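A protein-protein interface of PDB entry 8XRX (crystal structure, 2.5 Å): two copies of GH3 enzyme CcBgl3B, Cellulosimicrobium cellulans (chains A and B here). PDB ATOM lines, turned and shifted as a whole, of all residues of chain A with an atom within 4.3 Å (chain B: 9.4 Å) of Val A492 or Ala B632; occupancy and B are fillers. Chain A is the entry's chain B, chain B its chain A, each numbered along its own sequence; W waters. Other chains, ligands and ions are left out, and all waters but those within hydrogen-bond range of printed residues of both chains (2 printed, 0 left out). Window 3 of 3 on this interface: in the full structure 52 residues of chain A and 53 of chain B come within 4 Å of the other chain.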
ATOM      1  N   LEU A 471      17.680 -25.027  -0.234  1.00  0.00           N
ATOM      2  CA  LEU A 471      17.069 -23.709  -0.191  1.00  0.00           C
ATOM      3  C   LEU A 471      15.778 -23.751   0.613  1.00  0.00           C
ATOM      4  O   LEU A 471      15.242 -24.812   0.924  1.00  0.00           O
ATOM      5  CB  LEU A 471      16.810 -23.180  -1.606  1.00  0.00           C
ATOM      6  CG  LEU A 471      15.904 -24.002  -2.549  1.00  0.00           C
ATOM      7  CD1 LEU A 471      14.432 -23.637  -2.431  1.00  0.00           C
ATOM      8  CD2 LEU A 471      16.332 -23.861  -3.971  1.00  0.00           C
ATOM      9  N   THR A 472      15.265 -22.562   0.855  1.00  0.00           N
ATOM     10  CA  THR A 472      13.922 -22.302   1.417  1.00  0.00           C
ATOM     11  C   THR A 472      13.355 -21.103   0.661  1.00  0.00           C
ATOM     12  O   THR A 472      14.125 -20.329   0.115  1.00  0.00           O
ATOM     13  CB  THR A 472      13.891 -22.084   2.930  1.00  0.00           C
ATOM     14  OG1 THR A 472      14.758 -21.020   3.292  1.00  0.00           O
ATOM     15  CG2 THR A 472      14.226 -23.328   3.710  1.00  0.00           C
ATOM     16  N   LEU A 473      12.040 -20.983   0.606  1.00  0.00           N
ATOM     17  CA  LEU A 473      11.476 -19.806  -0.081  1.00  0.00           C
ATOM     18  C   LEU A 473      11.076 -18.741   0.938  1.00  0.00           C
ATOM     19  O   LEU A 473      10.896 -19.064   2.092  1.00  0.00           O
ATOM     20  CB  LEU A 473      10.319 -20.263  -0.960  1.00  0.00           C
ATOM     21  CG  LEU A 473      10.769 -21.082  -2.161  1.00  0.00           C
ATOM     22  CD1 LEU A 473       9.599 -21.755  -2.829  1.00  0.00           C
ATOM     23  CD2 LEU A 473      11.508 -20.206  -3.143  1.00  0.00           C
ATOM     24  N   VAL A 491      11.111 -15.601  -3.463  1.00  0.00           N
ATOM     25  CA  VAL A 491      12.538 -15.643  -3.767  1.00  0.00           C
ATOM     26  C   VAL A 491      13.206 -16.793  -3.031  1.00  0.00           C
ATOM     27  O   VAL A 491      12.779 -17.211  -1.951  1.00  0.00           O
ATOM     28  CB  VAL A 491      13.249 -14.323  -3.418  1.00  0.00           C
ATOM     29  CG1 VAL A 491      12.713 -13.202  -4.280  1.00  0.00           C
ATOM     30  CG2 VAL A 491      13.068 -14.004  -1.958  1.00  0.00           C
ATOM     31  N   VAL A 492      14.280 -17.292  -3.630  1.00  0.00           N
ATOM     32  CA  VAL A 492      15.060 -18.378  -3.054  1.00  0.00           C
ATOM     33  C   VAL A 492      15.946 -17.814  -1.954  1.00  0.00           C
ATOM     34  O   VAL A 492      16.585 -16.776  -2.136  1.00  0.00           O
ATOM     35  CB  VAL A 492      15.892 -19.075  -4.140  1.00  0.00           C
ATOM     36  CG1 VAL A 492      16.834 -20.095  -3.544  1.00  0.00           C
ATOM     37  CG2 VAL A 492      14.989 -19.742  -5.124  1.00  0.00           C
ATOM     38  N   VAL A 493      15.962 -18.473  -0.805  1.00  0.00           N
ATOM     39  CA  VAL A 493      16.967 -18.222   0.222  1.00  0.00           C
ATOM     40  C   VAL A 493      17.850 -19.458   0.299  1.00  0.00           C
ATOM     41  O   VAL A 493      17.358 -20.538   0.635  1.00  0.00           O
ATOM     42  CB  VAL A 493      16.345 -17.911   1.591  1.00  0.00           C
ATOM     43  CG1 VAL A 493      17.392 -17.321   2.488  1.00  0.00           C
ATOM     44  CG2 VAL A 493      15.200 -16.953   1.459  1.00  0.00           C
ATOM     45  N   PRO A 494      19.127 -19.370  -0.039  1.00  0.00           N
ATOM     46  CA  PRO A 494      19.984 -20.551   0.073  1.00  0.00           C
ATOM     47  C   PRO A 494      20.111 -20.992   1.526  1.00  0.00           C
ATOM     48  O   PRO A 494      20.293 -20.178   2.428  1.00  0.00           O
ATOM     49  CB  PRO A 494      21.326 -20.070  -0.499  1.00  0.00           C
ATOM     50  CG  PRO A 494      20.980 -18.924  -1.359  1.00  0.00           C
ATOM     51  CD  PRO A 494      19.796 -18.260  -0.731  1.00  0.00           C
ATOM     52  N   GLU A 524      12.953 -24.858  -7.965  1.00  0.00           N
ATOM     53  CA  GLU A 524      12.937 -23.408  -7.816  1.00  0.00           C
ATOM     54  C   GLU A 524      14.149 -22.718  -8.429  1.00  0.00           C
ATOM     55  O   GLU A 524      14.168 -21.487  -8.473  1.00  0.00           O
ATOM     56  CB  GLU A 524      12.856 -23.018  -6.344  1.00  0.00           C
ATOM     57  CG  GLU A 524      11.638 -23.480  -5.600  1.00  0.00           C
ATOM     58  CD  GLU A 524      11.814 -24.840  -4.989  1.00  0.00           C
ATOM     59  OE1 GLU A 524      12.897 -25.427  -5.125  1.00  0.00           O
ATOM     60  OE2 GLU A 524      10.856 -25.338  -4.382  1.00  0.00           O
ATOM     61  N   LEU A 525      15.163 -23.470  -8.871  1.00  0.00           N
ATOM     62  CA  LEU A 525      16.356 -22.941  -9.517  1.00  0.00           C
ATOM     63  C   LEU A 525      16.407 -23.266 -11.013  1.00  0.00           C
ATOM     64  O   LEU A 525      17.467 -23.184 -11.633  1.00  0.00           O
ATOM     65  CB  LEU A 525      17.589 -23.494  -8.812  1.00  0.00           C
ATOM     66  CG  LEU A 525      17.782 -23.132  -7.335  1.00  0.00           C
ATOM     67  CD1 LEU A 525      18.681 -24.136  -6.654  1.00  0.00           C
ATOM     68  CD2 LEU A 525      18.321 -21.726  -7.175  1.00  0.00           C
ATOM     69  N   ARG A 530      13.415 -18.384 -14.205  1.00  0.00           N
ATOM     70  CA  ARG A 530      14.351 -18.812 -13.178  1.00  0.00           C
ATOM     71  C   ARG A 530      15.711 -19.157 -13.782  1.00  0.00           C
ATOM     72  O   ARG A 530      16.278 -20.217 -13.539  1.00  0.00           O
ATOM     73  CB  ARG A 530      13.794 -19.994 -12.388  1.00  0.00           C
ATOM     74  CG  ARG A 530      12.658 -19.638 -11.485  1.00  0.00           C
ATOM     75  CD  ARG A 530      11.870 -20.848 -11.115  1.00  0.00           C
ATOM     76  NE  ARG A 530      11.080 -21.307 -12.249  1.00  0.00           N
ATOM     77  CZ  ARG A 530      10.313 -22.393 -12.237  1.00  0.00           C
ATOM     78  NH1 ARG A 530       9.621 -22.735 -13.321  1.00  0.00           N
ATOM     79  NH2 ARG A 530      10.249 -23.140 -11.139  1.00  0.00           N
ATOM     80  N   SER A 531      16.257 -18.251 -14.578  1.00  0.00           N
ATOM     81  CA  SER A 531      17.658 -18.335 -14.925  1.00  0.00           C
ATOM     82  C   SER A 531      18.516 -18.114 -13.674  1.00  0.00           C
ATOM     83  O   SER A 531      18.064 -17.550 -12.686  1.00  0.00           O
ATOM     84  CB  SER A 531      18.003 -17.294 -15.982  1.00  0.00           C
ATOM     85  OG  SER A 531      17.087 -17.286 -17.036  1.00  0.00           O
ATOM     86  N   THR A 532      19.757 -18.582 -13.721  1.00  0.00           N
ATOM     87  CA  THR A 532      20.698 -18.453 -12.616  1.00  0.00           C
ATOM     88  C   THR A 532      21.946 -17.707 -13.059  1.00  0.00           C
ATOM     89  O   THR A 532      22.383 -17.831 -14.196  1.00  0.00           O
ATOM     90  CB  THR A 532      21.137 -19.796 -12.048  1.00  0.00           C
ATOM     91  OG1 THR A 532      21.693 -20.601 -13.082  1.00  0.00           O
ATOM     92  CG2 THR A 532      20.002 -20.511 -11.381  1.00  0.00           C
ATOM     93  N   GLN B 626      11.960  -8.830 -20.322  1.00  0.00           N
ATOM     94  CA  GLN B 626      12.260 -10.020 -19.543  1.00  0.00           C
ATOM     95  C   GLN B 626      11.021 -10.540 -18.811  1.00  0.00           C
ATOM     96  O   GLN B 626      10.225  -9.765 -18.282  1.00  0.00           O
ATOM     97  CB  GLN B 626      13.384  -9.699 -18.560  1.00  0.00           C
ATOM     98  CG  GLN B 626      13.857 -10.872 -17.748  1.00  0.00           C
ATOM     99  CD  GLN B 626      14.841 -10.498 -16.640  1.00  0.00           C
ATOM    100  OE1 GLN B 626      15.207  -9.343 -16.472  1.00  0.00           O
ATOM    101  NE2 GLN B 626      15.243 -11.483 -15.875  1.00  0.00           N
ATOM    102  N   HIS B 627      10.847 -11.865 -18.820  1.00  0.00           N
ATOM    103  CA  HIS B 627       9.934 -12.568 -17.919  1.00  0.00           C
ATOM    104  C   HIS B 627      10.653 -12.743 -16.595  1.00  0.00           C
ATOM    105  O   HIS B 627      11.481 -13.643 -16.448  1.00  0.00           O
ATOM    106  CB  HIS B 627       9.540 -13.949 -18.443  1.00  0.00           C
ATOM    107  CG  HIS B 627       8.893 -13.963 -19.787  1.00  0.00           C
ATOM    108  ND1 HIS B 627       8.768 -12.845 -20.580  1.00  0.00           N
ATOM    109  CD2 HIS B 627       8.347 -14.981 -20.486  1.00  0.00           C
ATOM    110  CE1 HIS B 627       8.161 -13.172 -21.702  1.00  0.00           C
ATOM    111  NE2 HIS B 627       7.905 -14.465 -21.673  1.00  0.00           N
ATOM    112  N   GLY B 628      10.322 -11.922 -15.614  1.00  0.00           N
ATOM    113  CA  GLY B 628      10.987 -11.952 -14.329  1.00  0.00           C
ATOM    114  C   GLY B 628      11.853 -10.722 -14.114  1.00  0.00           C
ATOM    115  O   GLY B 628      12.057  -9.898 -15.001  1.00  0.00           O
ATOM    116  N   VAL B 629      12.350 -10.609 -12.885  1.00  0.00           N
ATOM    117  CA  VAL B 629      13.114  -9.452 -12.435  1.00  0.00           C
ATOM    118  C   VAL B 629      14.430  -9.863 -11.780  1.00  0.00           C
ATOM    119  O   VAL B 629      15.251  -9.007 -11.457  1.00  0.00           O
ATOM    120  CB  VAL B 629      12.293  -8.594 -11.450  1.00  0.00           C
ATOM    121  CG1 VAL B 629      10.988  -8.201 -12.043  1.00  0.00           C
ATOM    122  CG2 VAL B 629      12.070  -9.330 -10.124  1.00  0.00           C
ATOM    123  N   ARG B 630      14.640 -11.157 -11.553  1.00  0.00           N
ATOM    124  CA  ARG B 630      15.822 -11.607 -10.838  1.00  0.00           C
ATOM    125  C   ARG B 630      16.225 -12.993 -11.303  1.00  0.00           C
ATOM    126  O   ARG B 630      15.416 -13.759 -11.811  1.00  0.00           O
ATOM    127  CB  ARG B 630      15.612 -11.635  -9.321  1.00  0.00           C
ATOM    128  CG  ARG B 630      14.395 -12.402  -8.877  1.00  0.00           C
ATOM    129  CD  ARG B 630      14.620 -13.105  -7.559  1.00  0.00           C
ATOM    130  NE  ARG B 630      15.326 -12.278  -6.578  1.00  0.00           N
ATOM    131  CZ  ARG B 630      16.361 -12.689  -5.854  1.00  0.00           C
ATOM    132  NH1 ARG B 630      16.825 -13.922  -5.981  1.00  0.00           N
ATOM    133  NH2 ARG B 630      16.922 -11.872  -4.986  1.00  0.00           N
ATOM    134  N   TYR B 631      17.504 -13.299 -11.127  1.00  0.00           N
ATOM    135  CA  TYR B 631      17.950 -14.670 -11.232  1.00  0.00           C
ATOM    136  C   TYR B 631      17.443 -15.448 -10.027  1.00  0.00           C
ATOM    137  O   TYR B 631      17.106 -14.885  -8.993  1.00  0.00           O
ATOM    138  CB  TYR B 631      19.477 -14.735 -11.338  1.00  0.00           C
ATOM    139  CG  TYR B 631      20.025 -14.076 -12.579  1.00  0.00           C
ATOM    140  CD1 TYR B 631      20.090 -14.765 -13.777  1.00  0.00           C
ATOM    141  CD2 TYR B 631      20.466 -12.767 -12.559  1.00  0.00           C
ATOM    142  CE1 TYR B 631      20.579 -14.171 -14.921  1.00  0.00           C
ATOM    143  CE2 TYR B 631      20.947 -12.170 -13.691  1.00  0.00           C
ATOM    144  CZ  TYR B 631      21.005 -12.876 -14.866  1.00  0.00           C
ATOM    145  OH  TYR B 631      21.478 -12.292 -15.998  1.00  0.00           O
ATOM    146  N   ALA B 632      17.359 -16.758 -10.176  1.00  0.00           N
ATOM    147  CA  ALA B 632      16.851 -17.545  -9.075  1.00  0.00           C
ATOM    148  C   ALA B 632      17.821 -17.567  -7.909  1.00  0.00           C
ATOM    149  O   ALA B 632      17.397 -17.806  -6.782  1.00  0.00           O
ATOM    150  CB  ALA B 632      16.537 -18.959  -9.544  1.00  0.00           C
ATOM    151  N   ASP B 633      19.102 -17.299  -8.153  1.00  0.00           N
ATOM    152  CA  ASP B 633      20.125 -17.285  -7.127  1.00  0.00           C
ATOM    153  C   ASP B 633      20.713 -15.902  -6.891  1.00  0.00           C
ATOM    154  O   ASP B 633      21.640 -15.773  -6.106  1.00  0.00           O
ATOM    155  CB  ASP B 633      21.232 -18.282  -7.476  1.00  0.00           C
ATOM    156  CG  ASP B 633      21.872 -18.022  -8.846  1.00  0.00           C
ATOM    157  OD1 ASP B 633      21.435 -17.115  -9.575  1.00  0.00           O
ATOM    158  OD2 ASP B 633      22.797 -18.758  -9.211  1.00  0.00           O
ATOM    159  N   LEU B 634      20.182 -14.859  -7.510  1.00  0.00           N
ATOM    160  CA  LEU B 634      20.824 -13.565  -7.353  1.00  0.00           C
ATOM    161  C   LEU B 634      19.906 -12.479  -7.881  1.00  0.00           C
ATOM    162  O   LEU B 634      19.262 -12.651  -8.917  1.00  0.00           O
ATOM    163  CB  LEU B 634      22.168 -13.512  -8.104  1.00  0.00           C
ATOM    164  CG  LEU B 634      23.124 -12.372  -7.752  1.00  0.00           C
ATOM    165  CD1 LEU B 634      23.807 -12.674  -6.463  1.00  0.00           C
ATOM    166  CD2 LEU B 634      24.140 -12.168  -8.821  1.00  0.00           C
ATOM    167  N   THR B 635      19.864 -11.365  -7.175  1.00  0.00           N
ATOM    168  CA  THR B 635      19.191 -10.188  -7.687  1.00  0.00           C
ATOM    169  C   THR B 635      19.892  -9.686  -8.956  1.00  0.00           C
ATOM    170  O   THR B 635      21.046  -9.998  -9.221  1.00  0.00           O
ATOM    171  CB  THR B 635      19.156  -9.103  -6.610  1.00  0.00           C
ATOM    172  OG1 THR B 635      18.427  -7.972  -7.073  1.00  0.00           O
ATOM    173  CG2 THR B 635      20.561  -8.655  -6.245  1.00  0.00           C
ATOM    174  N   GLN B 636      19.160  -8.917  -9.754  1.00  0.00           N
ATOM    175  CA  GLN B 636      19.709  -8.219 -10.902  1.00  0.00           C
ATOM    176  C   GLN B 636      20.017  -6.776 -10.583  1.00  0.00           C
ATOM    177  O   GLN B 636      20.508  -6.050 -11.440  1.00  0.00           O
ATOM    178  CB  GLN B 636      18.754  -8.309 -12.097  1.00  0.00           C
ATOM    179  CG  GLN B 636      18.589  -9.722 -12.588  1.00  0.00           C
ATOM    180  CD  GLN B 636      17.613  -9.887 -13.732  1.00  0.00           C
ATOM    181  OE1 GLN B 636      17.141 -10.987 -13.977  1.00  0.00           O
ATOM    182  NE2 GLN B 636      17.328  -8.822 -14.440  1.00  0.00           N
HETATM  183  O   HOH W   1      14.958 -16.319  -6.438  1.00  0.00           O
HETATM  184  O   HOH W   2      15.217 -15.577 -14.354  1.00  0.00           O
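The backbone NH (N) of Ala B632 sits at hydrogen-bond distance from the backbone carbonyl oxygen (O) of Ser A531, at 2.7 Å.
The backbone NH of Arg B630 sits close to the side-chain amide oxygen of Gln B636 (3.5 Å).
Among the printed residues, merely in contact across the chains: Ser A531 with Tyr B631 (3.2 Å), Val A492 with Ala B632 (3.3 Å), Thr A532 with Asp B633 (3.4 Å), Thr A532 with Tyr B631 (3.6 Å), Val A491 with Arg B630 (3.6 Å), Glu A524 with Ala B632 (3.6 Å) and Leu A525 with Ala B632 (3.99 Å).
Val A492 touches just one residue of chain B: Ala B632 (3.3 Å). Printed residues of chain A within 4 Å of Ala B632: Val A492 (3.3 Å), Glu A524 (3.6 Å), Leu A525 (3.99 Å) and Ser A531 (2.7 Å). Val A491 touches one residue of chain B. Of the printed residues of chain B, Thr A532 touches Tyr B631 and Asp B633. Of the printed residues of chain B, Glu A524 touches Ala B632 (3.6 Å). Of the printed residues of chain B, Leu A525 touches Ala B632 (3.99 Å). Printed residues of chain A within 4 Å of Tyr B631: Ser A531 and Thr A532. Of the printed residues of chain A, Arg B630 touches Val A491. Gln B626 touches none of the printed residues of chain A. Leu B634 touches none of the printed residues of chain A. The nearest residue of chain B that does not touch Val A492 is Arg B630 (4.8 Å).
Printed residues of chain A that touch a printed residue of chain B: Val A491, Val A492, Glu A524, Leu A525, Ser A531 and Thr A532. Hydrophobic or aromatic side chains of chain A that line the printed part of chain B: Val A491 and Val A492.
No position is printed for both chains. Of the 8 pairs that touch across the chains among the printed residues, none has its exchanged pair printed and touching as well.
Water W1 lies within hydrogen-bond range of O of Ala B632 (2.9 Å), N of Val A492 (3.0 Å) and NH1 of Arg B630 (3.1 Å). Water W2 lies within hydrogen-bond range of N of Ser A531 (2.9 Å), O of Arg B630 (3.1 Å) and N of Arg A530 (3.3 Å).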
